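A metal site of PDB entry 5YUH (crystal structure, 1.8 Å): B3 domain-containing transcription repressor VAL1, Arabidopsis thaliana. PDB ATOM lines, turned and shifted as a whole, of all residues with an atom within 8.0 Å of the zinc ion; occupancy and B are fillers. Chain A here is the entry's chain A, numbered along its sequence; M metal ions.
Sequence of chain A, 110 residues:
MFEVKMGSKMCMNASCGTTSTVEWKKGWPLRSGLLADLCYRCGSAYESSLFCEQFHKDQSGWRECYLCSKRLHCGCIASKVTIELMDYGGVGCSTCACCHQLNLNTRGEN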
ATOM      1  N   GLU A  64     -21.277  26.508 -28.326  1.00  0.00           N
ATOM      2  CA  GLU A  64     -19.951  25.951 -28.195  1.00  0.00           C
ATOM      3  C   GLU A  64     -19.201  26.722 -27.130  1.00  0.00           C
ATOM      4  O   GLU A  64     -19.296  27.948 -27.088  1.00  0.00           O
ATOM      5  CB  GLU A  64     -19.218  26.012 -29.542  1.00  0.00           C
ATOM      6  CG  GLU A  64     -19.818  25.074 -30.560  1.00  0.00           C
ATOM      7  CD  GLU A  64     -19.113  25.126 -31.904  1.00  0.00           C
ATOM      8  OE1 GLU A  64     -18.230  25.994 -32.089  1.00  0.00           O
ATOM      9  OE2 GLU A  64     -19.435  24.288 -32.764  1.00  0.00           O
ATOM     10  N   CYS A  65     -18.497  26.000 -26.246  1.00  0.00           N
ATOM     11  CA  CYS A  65     -17.607  26.628 -25.275  1.00  0.00           C
ATOM     12  C   CYS A  65     -16.677  27.590 -25.979  1.00  0.00           C
ATOM     13  O   CYS A  65     -16.103  27.268 -27.028  1.00  0.00           O
ATOM     14  CB  CYS A  65     -16.784  25.568 -24.535  1.00  0.00           C
ATOM     15  SG  CYS A  65     -15.544  26.266 -23.421  1.00  0.00           S
ATOM     16  N   TYR A  66     -16.485  28.773 -25.380  1.00  0.00           N
ATOM     17  CA  TYR A  66     -15.683  29.796 -26.025  1.00  0.00           C
ATOM     18  C   TYR A  66     -14.215  29.383 -26.152  1.00  0.00           C
ATOM     19  O   TYR A  66     -13.480  29.991 -26.945  1.00  0.00           O
ATOM     20  CB  TYR A  66     -15.775  31.110 -25.238  1.00  0.00           C
ATOM     21  CG  TYR A  66     -14.864  31.112 -24.051  1.00  0.00           C
ATOM     22  CD1 TYR A  66     -15.225  30.465 -22.874  1.00  0.00           C
ATOM     23  CD2 TYR A  66     -13.619  31.730 -24.109  1.00  0.00           C
ATOM     24  CE1 TYR A  66     -14.371  30.452 -21.787  1.00  0.00           C
ATOM     25  CE2 TYR A  66     -12.765  31.716 -23.023  1.00  0.00           C
ATOM     26  CZ  TYR A  66     -13.140  31.074 -21.865  1.00  0.00           C
ATOM     27  OH  TYR A  66     -12.285  31.054 -20.786  1.00  0.00           O
ATOM     28  N   LEU A  67     -13.766  28.382 -25.403  1.00  0.00           N
ATOM     29  CA  LEU A  67     -12.340  28.054 -25.371  1.00  0.00           C
ATOM     30  C   LEU A  67     -12.008  26.681 -25.924  1.00  0.00           C
ATOM     31  O   LEU A  67     -11.017  26.545 -26.639  1.00  0.00           O
ATOM     32  CB  LEU A  67     -11.788  28.175 -23.945  1.00  0.00           C
ATOM     33  CG  LEU A  67     -10.294  27.877 -23.756  1.00  0.00           C
ATOM     34  CD1 LEU A  67      -9.466  28.670 -24.757  1.00  0.00           C
ATOM     35  CD2 LEU A  67      -9.853  28.163 -22.316  1.00  0.00           C
ATOM     36  N   CYS A  68     -12.803  25.661 -25.636  1.00  0.00           N
ATOM     37  CA  CYS A  68     -12.500  24.328 -26.148  1.00  0.00           C
ATOM     38  C   CYS A  68     -13.487  23.855 -27.201  1.00  0.00           C
ATOM     39  O   CYS A  68     -13.337  22.744 -27.728  1.00  0.00           O
ATOM     40  CB  CYS A  68     -12.461  23.320 -24.998  1.00  0.00           C
ATOM     41  SG  CYS A  68     -14.091  22.869 -24.389  1.00  0.00           S
ATOM     42  N   SER A  69     -14.512  24.648 -27.497  1.00  0.00           N
ATOM     43  CA  SER A  69     -15.526  24.349 -28.502  1.00  0.00           C
ATOM     44  C   SER A  69     -16.428  23.175 -28.167  1.00  0.00           C
ATOM     45  O   SER A  69     -17.245  22.801 -28.999  1.00  0.00           O
ATOM     46  CB  SER A  69     -14.920  24.124 -29.892  1.00  0.00           C
ATOM     47  OG  SER A  69     -14.281  25.298 -30.347  1.00  0.00           O
ATOM     48  N   LYS A  70     -16.323  22.590 -26.968  1.00  0.00           N
ATOM     49  CA  LYS A  70     -17.286  21.581 -26.532  1.00  0.00           C
ATOM     50  C   LYS A  70     -18.707  22.074 -26.756  1.00  0.00           C
ATOM     51  O   LYS A  70     -19.007  23.238 -26.523  1.00  0.00           O
ATOM     52  CB  LYS A  70     -17.095  21.280 -25.058  1.00  0.00           C
ATOM     53  CG  LYS A  70     -17.849  20.073 -24.606  1.00  0.00           C
ATOM     54  CD  LYS A  70     -17.770  19.908 -23.106  1.00  0.00           C
ATOM     55  CE  LYS A  70     -18.448  18.633 -22.729  1.00  0.00           C
ATOM     56  NZ  LYS A  70     -18.274  18.351 -21.273  1.00  0.00           N
ATOM     57  N   ARG A  71     -19.589  21.175 -27.193  1.00  0.00           N
ATOM     58  CA  ARG A  71     -21.013  21.498 -27.340  1.00  0.00           C
ATOM     59  C   ARG A  71     -21.708  21.528 -25.971  1.00  0.00           C
ATOM     60  O   ARG A  71     -21.584  20.576 -25.184  1.00  0.00           O
ATOM     61  CB  ARG A  71     -21.678  20.490 -28.269  1.00  0.00           C
ATOM     62  CG  ARG A  71     -21.402  20.700 -29.750  1.00  0.00           C
ATOM     63  CD  ARG A  71     -22.510  20.157 -30.657  1.00  0.00           C
ATOM     64  NE  ARG A  71     -23.132  21.294 -31.338  1.00  0.00           N
ATOM     65  CZ  ARG A  71     -24.416  21.365 -31.697  1.00  0.00           C
ATOM     66  NH1 ARG A  71     -24.894  22.482 -32.259  1.00  0.00           N
ATOM     67  NH2 ARG A  71     -25.233  20.321 -31.486  1.00  0.00           N
ATOM     68  N   LEU A  72     -22.414  22.627 -25.682  1.00  0.00           N
ATOM     69  CA  LEU A  72     -23.075  22.866 -24.393  1.00  0.00           C
ATOM     70  C   LEU A  72     -24.545  23.162 -24.657  1.00  0.00           C
ATOM     71  O   LEU A  72     -24.860  24.051 -25.447  1.00  0.00           O
ATOM     72  CB  LEU A  72     -22.443  24.052 -23.672  1.00  0.00           C
ATOM     73  CG  LEU A  72     -20.950  23.905 -23.347  1.00  0.00           C
ATOM     74  CD1 LEU A  72     -20.413  25.241 -22.822  1.00  0.00           C
ATOM     75  CD2 LEU A  72     -20.807  22.786 -22.349  1.00  0.00           C
ATOM     76  N   THR A  82     -23.319  22.718 -15.420  1.00  0.00           N
ATOM     77  CA  THR A  82     -22.051  22.537 -16.118  1.00  0.00           C
ATOM     78  C   THR A  82     -21.723  23.674 -17.082  1.00  0.00           C
ATOM     79  O   THR A  82     -20.697  23.598 -17.777  1.00  0.00           O
ATOM     80  CB  THR A  82     -22.051  21.217 -16.902  1.00  0.00           C
ATOM     81  OG1 THR A  82     -23.142  21.230 -17.841  1.00  0.00           O
ATOM     82  CG2 THR A  82     -22.217  20.020 -15.980  1.00  0.00           C
ATOM     83  N   VAL A  91     -20.646  31.167 -23.760  1.00  0.00           N
ATOM     84  CA  VAL A  91     -20.605  30.251 -22.634  1.00  0.00           C
ATOM     85  C   VAL A  91     -19.248  29.568 -22.576  1.00  0.00           C
ATOM     86  O   VAL A  91     -18.495  29.539 -23.566  1.00  0.00           O
ATOM     87  CB  VAL A  91     -21.715  29.187 -22.691  1.00  0.00           C
ATOM     88  CG1 VAL A  91     -23.099  29.808 -22.356  1.00  0.00           C
ATOM     89  CG2 VAL A  91     -21.718  28.485 -24.064  1.00  0.00           C
ATOM     90  N   GLY A  92     -18.957  29.018 -21.403  1.00  0.00           N
ATOM     91  CA  GLY A  92     -17.781  28.176 -21.226  1.00  0.00           C
ATOM     92  C   GLY A  92     -18.125  26.996 -20.348  1.00  0.00           C
ATOM     93  O   GLY A  92     -18.986  27.069 -19.465  1.00  0.00           O
ATOM     94  N   CYS A  93     -17.471  25.859 -20.626  1.00  0.00           N
ATOM     95  CA  CYS A  93     -17.426  24.779 -19.651  1.00  0.00           C
ATOM     96  C   CYS A  93     -17.050  25.319 -18.292  1.00  0.00           C
ATOM     97  O   CYS A  93     -16.333  26.313 -18.173  1.00  0.00           O
ATOM     98  CB  CYS A  93     -16.399  23.725 -20.045  1.00  0.00           C
ATOM     99  SG  CYS A  93     -16.613  23.060 -21.642  1.00  0.00           S
ATOM    100  N   SER A  94     -17.484  24.631 -17.237  1.00  0.00           N
ATOM    101  CA  SER A  94     -17.010  24.980 -15.898  1.00  0.00           C
ATOM    102  C   SER A  94     -15.487  24.966 -15.826  1.00  0.00           C
ATOM    103  O   SER A  94     -14.890  25.830 -15.181  1.00  0.00           O
ATOM    104  CB  SER A  94     -17.624  24.048 -14.863  1.00  0.00           C
ATOM    105  OG  SER A  94     -19.019  24.279 -14.782  1.00  0.00           O
ATOM    106  N   THR A  95     -14.844  24.014 -16.514  1.00  0.00           N
ATOM    107  CA  THR A  95     -13.387  23.957 -16.601  1.00  0.00           C
ATOM    108  C   THR A  95     -12.792  25.226 -17.210  1.00  0.00           C
ATOM    109  O   THR A  95     -11.900  25.858 -16.638  1.00  0.00           O
ATOM    110  CB  THR A  95     -12.967  22.754 -17.454  1.00  0.00           C
ATOM    111  OG1 THR A  95     -13.636  21.585 -16.981  1.00  0.00           O
ATOM    112  CG2 THR A  95     -11.458  22.562 -17.432  1.00  0.00           C
ATOM    113  N   CYS A  96     -13.247  25.576 -18.425  1.00  0.00           N
ATOM    114  CA  CYS A  96     -12.639  26.647 -19.195  1.00  0.00           C
ATOM    115  C   CYS A  96     -13.024  28.032 -18.714  1.00  0.00           C
ATOM    116  O   CYS A  96     -12.305  28.994 -19.004  1.00  0.00           O
ATOM    117  CB  CYS A  96     -13.031  26.504 -20.669  1.00  0.00           C
ATOM    118  SG  CYS A  96     -12.773  24.852 -21.341  1.00  0.00           S
ATOM    119  N   ALA A  97     -14.144  28.176 -18.013  1.00  0.00           N
ATOM    120  CA  ALA A  97     -14.495  29.495 -17.496  1.00  0.00           C
ATOM    121  C   ALA A  97     -13.772  29.809 -16.194  1.00  0.00           C
ATOM    122  O   ALA A  97     -13.394  30.958 -15.945  1.00  0.00           O
ATOM    123  CB  ALA A  97     -16.000  29.603 -17.302  1.00  0.00           C
HETATM  124 ZN    ZN M   1     -14.595  24.292 -22.625  1.00  0.00          ZN
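O of Cys 96 is in hydrogen-bond range of OH of Tyr 66 (2.7 Å).
The backbone NH (N) of Leu 67 sits close to the side-chain sulfur (SG) of Cys 65, at 3.4 Å.
The backbone NH (N) of Cys 65 sits at hydrogen-bond distance from the backbone carbonyl oxygen (O) of Lys 70 (2.8 Å).
The side-chain sulfur of Cys 68 sits close to the backbone NH of Lys 70.
Of the 17 residues printed, 4 come within 4 Å of the zinc ion.
The nearest printed residue that does not touch the zinc ion is Lys 70 (4.6 Å).
The zinc ion is bound by the side-chain sulfur of Cys 96 (2.3 Å), the side-chain sulfur of Cys 68 (2.3 Å), the side-chain sulfur of Cys 65 (2.3 Å) and the side-chain sulfur of Cys 93 (2.6 Å).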
